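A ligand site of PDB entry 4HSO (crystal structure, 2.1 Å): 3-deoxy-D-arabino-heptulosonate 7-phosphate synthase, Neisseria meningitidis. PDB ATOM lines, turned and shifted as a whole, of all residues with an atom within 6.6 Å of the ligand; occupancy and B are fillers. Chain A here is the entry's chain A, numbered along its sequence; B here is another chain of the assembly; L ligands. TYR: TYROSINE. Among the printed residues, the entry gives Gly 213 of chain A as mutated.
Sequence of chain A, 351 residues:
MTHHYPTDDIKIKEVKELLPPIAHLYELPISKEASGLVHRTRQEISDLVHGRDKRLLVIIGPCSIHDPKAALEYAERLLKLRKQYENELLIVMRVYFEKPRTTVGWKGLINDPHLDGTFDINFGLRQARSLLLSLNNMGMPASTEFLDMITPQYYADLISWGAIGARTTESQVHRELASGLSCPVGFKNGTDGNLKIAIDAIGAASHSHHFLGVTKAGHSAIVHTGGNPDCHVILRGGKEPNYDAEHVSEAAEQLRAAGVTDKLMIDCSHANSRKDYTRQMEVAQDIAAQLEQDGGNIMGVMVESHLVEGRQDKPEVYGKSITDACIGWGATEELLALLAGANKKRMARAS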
ATOM      1  N   ARG A  42     -26.001 -22.610  35.433  1.00  0.00           N
ATOM      2  CA  ARG A  42     -27.004 -21.600  35.125  1.00  0.00           C
ATOM      3  C   ARG A  42     -28.305 -21.932  35.888  1.00  0.00           C
ATOM      4  O   ARG A  42     -28.911 -21.045  36.507  1.00  0.00           O
ATOM      5  CB  ARG A  42     -27.259 -21.472  33.633  1.00  0.00           C
ATOM      6  CG  ARG A  42     -26.065 -20.906  32.870  1.00  0.00           C
ATOM      7  CD  ARG A  42     -26.290 -21.024  31.357  1.00  0.00           C
ATOM      8  NE  ARG A  42     -25.312 -20.303  30.591  1.00  0.00           N
ATOM      9  CZ  ARG A  42     -25.272 -20.320  29.250  1.00  0.00           C
ATOM     10  NH1 ARG A  42     -26.139 -21.008  28.560  1.00  0.00           N
ATOM     11  NH2 ARG A  42     -24.379 -19.628  28.607  1.00  0.00           N
ATOM     12  N   PHE A 146     -20.075  -8.516  30.793  1.00  0.00           N
ATOM     13  CA  PHE A 146     -20.346  -8.238  29.378  1.00  0.00           C
ATOM     14  C   PHE A 146     -20.426  -6.738  29.159  1.00  0.00           C
ATOM     15  O   PHE A 146     -21.378  -6.076  29.570  1.00  0.00           O
ATOM     16  CB  PHE A 146     -21.655  -8.879  28.973  1.00  0.00           C
ATOM     17  CG  PHE A 146     -21.619 -10.339  28.952  1.00  0.00           C
ATOM     18  CD1 PHE A 146     -20.923 -10.997  27.959  1.00  0.00           C
ATOM     19  CD2 PHE A 146     -22.216 -11.065  29.920  1.00  0.00           C
ATOM     20  CE1 PHE A 146     -20.884 -12.376  27.913  1.00  0.00           C
ATOM     21  CE2 PHE A 146     -22.224 -12.448  29.871  1.00  0.00           C
ATOM     22  CZ  PHE A 146     -21.515 -13.099  28.898  1.00  0.00           C
ATOM     23  N   MET A 149     -21.173  -5.232  22.947  1.00  0.00           N
ATOM     24  CA  MET A 149     -22.315  -5.933  22.341  1.00  0.00           C
ATOM     25  C   MET A 149     -21.925  -7.139  21.451  1.00  0.00           C
ATOM     26  O   MET A 149     -22.753  -8.019  21.234  1.00  0.00           O
ATOM     27  CB  MET A 149     -23.101  -4.956  21.482  1.00  0.00           C
ATOM     28  CG  MET A 149     -23.680  -3.768  22.218  1.00  0.00           C
ATOM     29  SD  MET A 149     -24.647  -4.325  23.654  1.00  0.00           S
ATOM     30  CE  MET A 149     -23.766  -3.518  24.942  1.00  0.00           C
ATOM     31  N   ILE A 150     -20.704  -7.176  20.925  1.00  0.00           N
ATOM     32  CA  ILE A 150     -20.309  -8.113  19.837  1.00  0.00           C
ATOM     33  C   ILE A 150     -19.512  -9.284  20.403  1.00  0.00           C
ATOM     34  O   ILE A 150     -19.747 -10.451  20.052  1.00  0.00           O
ATOM     35  CB  ILE A 150     -19.579  -7.339  18.717  1.00  0.00           C
ATOM     36  CG1 ILE A 150     -20.602  -6.472  17.967  1.00  0.00           C
ATOM     37  CG2 ILE A 150     -18.899  -8.283  17.743  1.00  0.00           C
ATOM     38  CD1 ILE A 150     -19.996  -5.570  16.942  1.00  0.00           C
ATOM     39  N   PRO A 152     -19.688 -11.042  23.206  1.00  0.00           N
ATOM     40  CA  PRO A 152     -20.390 -12.231  23.732  1.00  0.00           C
ATOM     41  C   PRO A 152     -20.626 -13.378  22.737  1.00  0.00           C
ATOM     42  O   PRO A 152     -20.769 -14.502  23.135  1.00  0.00           O
ATOM     43  CB  PRO A 152     -21.779 -11.657  24.116  1.00  0.00           C
ATOM     44  CG  PRO A 152     -21.547 -10.189  24.324  1.00  0.00           C
ATOM     45  CD  PRO A 152     -20.490  -9.799  23.372  1.00  0.00           C
ATOM     46  N   GLN A 153     -20.809 -13.102  21.452  1.00  0.00           N
ATOM     47  CA  GLN A 153     -21.068 -14.170  20.521  1.00  0.00           C
ATOM     48  C   GLN A 153     -19.865 -15.154  20.449  1.00  0.00           C
ATOM     49  O   GLN A 153     -20.013 -16.312  20.056  1.00  0.00           O
ATOM     50  CB  GLN A 153     -21.415 -13.593  19.118  1.00  0.00           C
ATOM     51  CG  GLN A 153     -22.816 -13.058  18.983  1.00  0.00           C
ATOM     52  CD  GLN A 153     -23.863 -14.185  18.824  1.00  0.00           C
ATOM     53  OE1 GLN A 153     -24.082 -14.978  19.734  1.00  0.00           O
ATOM     54  NE2 GLN A 153     -24.553 -14.200  17.706  1.00  0.00           N
ATOM     55  N   ALA A 156     -20.056 -16.493  25.077  1.00  0.00           N
ATOM     56  CA  ALA A 156     -21.165 -16.528  26.085  1.00  0.00           C
ATOM     57  C   ALA A 156     -21.589 -17.958  26.383  1.00  0.00           C
ATOM     58  O   ALA A 156     -22.111 -18.267  27.463  1.00  0.00           O
ATOM     59  CB  ALA A 156     -22.375 -15.757  25.599  1.00  0.00           C
ATOM     60  N   ASP A 157     -21.441 -18.834  25.380  1.00  0.00           N
ATOM     61  CA  ASP A 157     -21.791 -20.274  25.593  1.00  0.00           C
ATOM     62  C   ASP A 157     -20.999 -20.934  26.719  1.00  0.00           C
ATOM     63  O   ASP A 157     -21.398 -21.993  27.234  1.00  0.00           O
ATOM     64  CB  ASP A 157     -21.665 -21.083  24.296  1.00  0.00           C
ATOM     65  CG  ASP A 157     -20.239 -21.052  23.733  1.00  0.00           C
ATOM     66  OD1 ASP A 157     -19.633 -19.984  23.741  1.00  0.00           O
ATOM     67  OD2 ASP A 157     -19.754 -22.092  23.238  1.00  0.00           O
ATOM     68  N   LEU A 177     -29.072  -6.460  25.664  1.00  0.00           N
ATOM     69  CA  LEU A 177     -28.145  -7.571  25.584  1.00  0.00           C
ATOM     70  C   LEU A 177     -28.480  -8.597  26.657  1.00  0.00           C
ATOM     71  O   LEU A 177     -28.540  -9.800  26.401  1.00  0.00           O
ATOM     72  CB  LEU A 177     -26.719  -7.061  25.834  1.00  0.00           C
ATOM     73  CG  LEU A 177     -25.654  -8.121  25.894  1.00  0.00           C
ATOM     74  CD1 LEU A 177     -25.606  -8.826  24.542  1.00  0.00           C
ATOM     75  CD2 LEU A 177     -24.298  -7.528  26.217  1.00  0.00           C
ATOM     76  N   GLY A 180     -31.198 -11.112  26.339  1.00  0.00           N
ATOM     77  CA  GLY A 180     -30.966 -12.193  25.419  1.00  0.00           C
ATOM     78  C   GLY A 180     -29.819 -13.105  25.796  1.00  0.00           C
ATOM     79  O   GLY A 180     -29.478 -13.996  25.028  1.00  0.00           O
ATOM     80  N   LEU A 181     -29.262 -12.935  26.994  1.00  0.00           N
ATOM     81  CA  LEU A 181     -28.152 -13.780  27.404  1.00  0.00           C
ATOM     82  C   LEU A 181     -28.700 -15.054  27.995  1.00  0.00           C
ATOM     83  O   LEU A 181     -29.735 -15.068  28.655  1.00  0.00           O
ATOM     84  CB  LEU A 181     -27.238 -13.080  28.411  1.00  0.00           C
ATOM     85  CG  LEU A 181     -26.313 -11.996  27.885  1.00  0.00           C
ATOM     86  CD1 LEU A 181     -25.585 -11.334  29.049  1.00  0.00           C
ATOM     87  CD2 LEU A 181     -25.309 -12.573  26.891  1.00  0.00           C
ATOM     88  N   SER A 182     -28.027 -16.130  27.729  1.00  0.00           N
ATOM     89  CA  SER A 182     -28.513 -17.424  28.169  1.00  0.00           C
ATOM     90  C   SER A 182     -28.201 -17.638  29.638  1.00  0.00           C
ATOM     91  O   SER A 182     -28.745 -18.542  30.225  1.00  0.00           O
ATOM     92  CB  SER A 182     -27.879 -18.528  27.301  1.00  0.00           C
ATOM     93  OG  SER A 182     -28.105 -18.263  25.921  1.00  0.00           O
ATOM     94  N   CYS A 183     -27.351 -16.809  30.219  1.00  0.00           N
ATOM     95  CA  CYS A 183     -27.028 -16.954  31.620  1.00  0.00           C
ATOM     96  C   CYS A 183     -27.849 -15.971  32.496  1.00  0.00           C
ATOM     97  O   CYS A 183     -28.268 -14.957  32.034  1.00  0.00           O
ATOM     98  CB  CYS A 183     -25.546 -16.742  31.834  1.00  0.00           C
ATOM     99  SG  CYS A 183     -24.910 -15.124  31.295  1.00  0.00           S
ATOM    100  N   PHE A 211     -33.335  -5.639  18.798  1.00  0.00           N
ATOM    101  CA  PHE A 211     -32.224  -4.725  18.601  1.00  0.00           C
ATOM    102  C   PHE A 211     -31.277  -5.273  17.531  1.00  0.00           C
ATOM    103  O   PHE A 211     -31.405  -6.428  17.104  1.00  0.00           O
ATOM    104  CB  PHE A 211     -31.473  -4.468  19.895  1.00  0.00           C
ATOM    105  CG  PHE A 211     -30.974  -5.700  20.518  1.00  0.00           C
ATOM    106  CD1 PHE A 211     -31.794  -6.448  21.335  1.00  0.00           C
ATOM    107  CD2 PHE A 211     -29.692  -6.150  20.283  1.00  0.00           C
ATOM    108  CE1 PHE A 211     -31.328  -7.615  21.912  1.00  0.00           C
ATOM    109  CE2 PHE A 211     -29.237  -7.301  20.820  1.00  0.00           C
ATOM    110  CZ  PHE A 211     -30.068  -8.043  21.643  1.00  0.00           C
ATOM    111  N   LEU A 212     -30.313  -4.460  17.171  1.00  0.00           N
ATOM    112  CA  LEU A 212     -29.367  -4.818  16.133  1.00  0.00           C
ATOM    113  C   LEU A 212     -28.190  -5.516  16.758  1.00  0.00           C
ATOM    114  O   LEU A 212     -27.614  -5.029  17.701  1.00  0.00           O
ATOM    115  CB  LEU A 212     -28.934  -3.593  15.391  1.00  0.00           C
ATOM    116  CG  LEU A 212     -30.081  -2.873  14.682  1.00  0.00           C
ATOM    117  CD1 LEU A 212     -29.451  -1.863  13.750  1.00  0.00           C
ATOM    118  CD2 LEU A 212     -30.992  -3.785  13.884  1.00  0.00           C
ATOM    119  N   GLY A 213     -27.866  -6.711  16.270  1.00  0.00           N
ATOM    120  CA  GLY A 213     -26.768  -7.496  16.841  1.00  0.00           C
ATOM    121  C   GLY A 213     -25.925  -8.056  15.711  1.00  0.00           C
ATOM    122  O   GLY A 213     -26.043  -7.627  14.560  1.00  0.00           O
ATOM    123  N   VAL A 214     -25.093  -9.023  16.031  1.00  0.00           N
ATOM    124  CA  VAL A 214     -24.221  -9.631  15.028  1.00  0.00           C
ATOM    125  C   VAL A 214     -24.359 -11.114  15.171  1.00  0.00           C
ATOM    126  O   VAL A 214     -24.425 -11.625  16.279  1.00  0.00           O
ATOM    127  CB  VAL A 214     -22.768  -9.181  15.148  1.00  0.00           C
ATOM    128  CG1 VAL A 214     -21.872  -9.811  14.075  1.00  0.00           C
ATOM    129  CG2 VAL A 214     -22.701  -7.671  14.956  1.00  0.00           C
ATOM    130  N   THR A 215     -24.510 -11.776  14.022  1.00  0.00           N
ATOM    131  CA  THR A 215     -24.606 -13.239  14.018  1.00  0.00           C
ATOM    132  C   THR A 215     -23.261 -13.926  14.232  1.00  0.00           C
ATOM    133  O   THR A 215     -22.244 -13.324  14.236  1.00  0.00           O
ATOM    134  CB  THR A 215     -25.131 -13.818  12.690  1.00  0.00           C
ATOM    135  OG1 THR A 215     -24.159 -13.672  11.674  1.00  0.00           O
ATOM    136  CG2 THR A 215     -26.426 -13.092  12.256  1.00  0.00           C
ATOM    137  N   LYS A 216     -23.314 -15.223  14.442  1.00  0.00           N
ATOM    138  CA  LYS A 216     -22.109 -16.018  14.623  1.00  0.00           C
ATOM    139  C   LYS A 216     -21.238 -15.995  13.421  1.00  0.00           C
ATOM    140  O   LYS A 216     -20.070 -16.269  13.533  1.00  0.00           O
ATOM    141  CB  LYS A 216     -22.505 -17.432  14.928  1.00  0.00           C
ATOM    142  CG  LYS A 216     -23.086 -17.410  16.320  1.00  0.00           C
ATOM    143  CD  LYS A 216     -23.123 -18.745  17.032  1.00  0.00           C
ATOM    144  CE  LYS A 216     -23.044 -18.547  18.552  1.00  0.00           C
ATOM    145  NZ  LYS A 216     -23.913 -17.454  19.090  1.00  0.00           N
ATOM    146  N   VAL A 223     -31.928  -8.979  16.165  1.00  0.00           N
ATOM    147  CA  VAL A 223     -32.081 -10.052  17.093  1.00  0.00           C
ATOM    148  C   VAL A 223     -33.293  -9.832  17.978  1.00  0.00           C
ATOM    149  O   VAL A 223     -33.521  -8.761  18.506  1.00  0.00           O
ATOM    150  CB  VAL A 223     -30.782 -10.333  17.890  1.00  0.00           C
ATOM    151  CG1 VAL A 223     -29.572 -10.481  16.977  1.00  0.00           C
ATOM    152  CG2 VAL A 223     -30.508  -9.252  18.853  1.00  0.00           C
ATOM    153  N   ASP B   8     -25.718 -22.038  22.699  1.00  0.00           N
ATOM    154  CA  ASP B   8     -26.035 -20.600  22.502  1.00  0.00           C
ATOM    155  C   ASP B   8     -27.547 -20.333  22.437  1.00  0.00           C
ATOM    156  O   ASP B   8     -28.430 -21.237  22.418  1.00  0.00           O
ATOM    157  CB  ASP B   8     -25.333 -20.064  21.203  1.00  0.00           C
ATOM    158  CG  ASP B   8     -23.976 -19.441  21.494  1.00  0.00           C
ATOM    159  OD1 ASP B   8     -23.984 -18.402  22.225  1.00  0.00           O
ATOM    160  OD2 ASP B   8     -22.930 -19.974  20.966  1.00  0.00           O
ATOM    161  N   ASP B   9     -27.825 -19.034  22.466  1.00  0.00           N
ATOM    162  CA  ASP B   9     -29.128 -18.490  22.100  1.00  0.00           C
ATOM    163  C   ASP B   9     -30.344 -19.052  22.886  1.00  0.00           C
ATOM    164  O   ASP B   9     -31.438 -19.155  22.326  1.00  0.00           O
ATOM    165  CB  ASP B   9     -29.306 -18.645  20.563  1.00  0.00           C
ATOM    166  CG  ASP B   9     -28.479 -17.621  19.757  1.00  0.00           C
ATOM    167  OD1 ASP B   9     -27.779 -16.783  20.358  1.00  0.00           O
ATOM    168  OD2 ASP B   9     -28.498 -17.669  18.506  1.00  0.00           O
ATOM    169  N   ILE B  10     -30.138 -19.411  24.164  1.00  0.00           N
ATOM    170  CA  ILE B  10     -31.219 -19.975  25.015  1.00  0.00           C
ATOM    171  C   ILE B  10     -32.456 -19.060  25.038  1.00  0.00           C
ATOM    172  O   ILE B  10     -33.587 -19.539  24.970  1.00  0.00           O
ATOM    173  CB  ILE B  10     -30.753 -20.213  26.487  1.00  0.00           C
ATOM    174  N   LYS B  11     -32.216 -17.755  25.129  1.00  0.00           N
ATOM    175  CA  LYS B  11     -33.302 -16.752  25.281  1.00  0.00           C
ATOM    176  C   LYS B  11     -33.415 -15.795  24.085  1.00  0.00           C
ATOM    177  O   LYS B  11     -33.859 -14.686  24.219  1.00  0.00           O
ATOM    178  CB  LYS B  11     -33.120 -15.992  26.584  1.00  0.00           C
ATOM    179  CG  LYS B  11     -33.272 -16.913  27.784  1.00  0.00           C
ATOM    180  CD  LYS B  11     -32.824 -16.223  29.069  1.00  0.00           C
ATOM    181  CE  LYS B  11     -32.096 -17.175  30.013  1.00  0.00           C
ATOM    182  NZ  LYS B  11     -31.233 -16.418  30.963  1.00  0.00           N
ATOM    183  N   ILE B  12     -33.023 -16.286  22.916  1.00  0.00           N
ATOM    184  CA  ILE B  12     -33.195 -15.569  21.638  1.00  0.00           C
ATOM    185  C   ILE B  12     -34.345 -16.258  20.845  1.00  0.00           C
ATOM    186  O   ILE B  12     -34.221 -17.409  20.434  1.00  0.00           O
ATOM    187  CB  ILE B  12     -31.904 -15.566  20.788  1.00  0.00           C
ATOM    188  CG1 ILE B  12     -30.726 -14.990  21.596  1.00  0.00           C
ATOM    189  CG2 ILE B  12     -32.111 -14.855  19.444  1.00  0.00           C
ATOM    190  CD1 ILE B  12     -30.737 -13.489  21.786  1.00  0.00           C
ATOM    191  N   VAL B  15     -33.651 -14.395  14.839  1.00  0.00           N
ATOM    192  CA  VAL B  15     -32.680 -13.505  14.203  1.00  0.00           C
ATOM    193  C   VAL B  15     -33.206 -13.196  12.762  1.00  0.00           C
ATOM    194  O   VAL B  15     -33.478 -14.126  12.000  1.00  0.00           O
ATOM    195  CB  VAL B  15     -31.268 -14.144  14.182  1.00  0.00           C
ATOM    196  CG1 VAL B  15     -30.261 -13.305  13.387  1.00  0.00           C
ATOM    197  CG2 VAL B  15     -30.746 -14.373  15.583  1.00  0.00           C
HETATM  198  N   TYR L   1     -25.166 -15.781  21.965  1.00  0.00           N
HETATM  199  CA  TYR L   1     -25.720 -15.079  23.205  1.00  0.00           C
HETATM  200  C   TYR L   1     -26.229 -16.066  24.253  1.00  0.00           C
HETATM  201  O   TYR L   1     -26.376 -15.764  25.448  1.00  0.00           O
HETATM  202  CB  TYR L   1     -26.901 -14.123  22.871  1.00  0.00           C
HETATM  203  CG  TYR L   1     -26.562 -12.991  21.927  1.00  0.00           C
HETATM  204  CD1 TYR L   1     -25.847 -11.886  22.369  1.00  0.00           C
HETATM  205  CD2 TYR L   1     -26.979 -13.043  20.589  1.00  0.00           C
HETATM  206  CE1 TYR L   1     -25.535 -10.839  21.493  1.00  0.00           C
HETATM  207  CE2 TYR L   1     -26.672 -12.017  19.708  1.00  0.00           C
HETATM  208  CZ  TYR L   1     -25.950 -10.918  20.154  1.00  0.00           C
HETATM  209  OH  TYR L   1     -25.649  -9.933  19.230  1.00  0.00           O
HETATM  210  OXT TYR L   1     -26.580 -17.186  23.899  1.00  0.00           O
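The side-chain amide oxygen of Gln 153 is in hydrogen-bond range of a nitrogen (N) of the ligand (2.6 Å).
The backbone NH (N) of Asp 9 of chain B lies within hydrogen-bond range of an oxygen (OXT) of the ligand (2.6 Å).
The side-chain carboxylate (OD1) of Asp 9 of chain B is in salt-bridge range of a nitrogen (N) of the ligand (3.2 Å).
The backbone NH (N) of Ser 182 is in hydrogen-bond range of an oxygen (O) of the ligand (2.8 Å).
An oxygen (OXT) of the ligand sits at hydrogen-bond distance from the side-chain hydroxyl (OG) of Ser 182, at 2.8 Å.
OD1 of Asp 8 of chain B lies within salt-bridge range of N of the ligand (2.9 Å).
The backbone NH of Val 214 sits at hydrogen-bond distance from an oxygen (OH) of the ligand (3.4 Å).
The backbone carbonyl oxygen (O) of Val 214 lies within hydrogen-bond range of the side-chain amide nitrogen (NE2) of Gln 153 (2.9 Å).
The side-chain amino group of Lys 216 is in hydrogen-bond range of the side-chain amide oxygen of Gln 153 (2.6 Å).
The backbone NH of Ile 10 of chain B is in hydrogen-bond range of the side-chain hydroxyl of Ser 182, at 2.9 Å.
NZ of Lys 11 of chain B is in hydrogen-bond range of O of Ser 182.
The side-chain carboxylate (OD1) of Asp 8 of chain B lies within salt-bridge range of the side-chain amino group (NZ) of Lys 216 (3.3 Å).
The side-chain amino group (NZ) of Lys 11 of chain B sits at hydrogen-bond distance from the backbone carbonyl oxygen (O) of Leu 181.
Met 149 touches the ligand (O to CE1, 3.97 Å).
Leu 177 touches the ligand.
Gly 180 touches the ligand (O to CB, 3.4 Å).
Leu 181 touches the ligand.
CA of Gly 213 touches OH of the ligand, 3.6 Å away.
NZ of Lys 216 touches N of the ligand, 3.6 Å away.
Ile 12 of chain B touches the ligand (CD1 to CD2, 3.97 Å).
Hydrophobic or aromatic side chains that line the ligand: Leu 177, Leu 181 and Ile 12 of chain B.
The nearest printed residue that does not touch the ligand is Ala 156 (4.004 Å).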
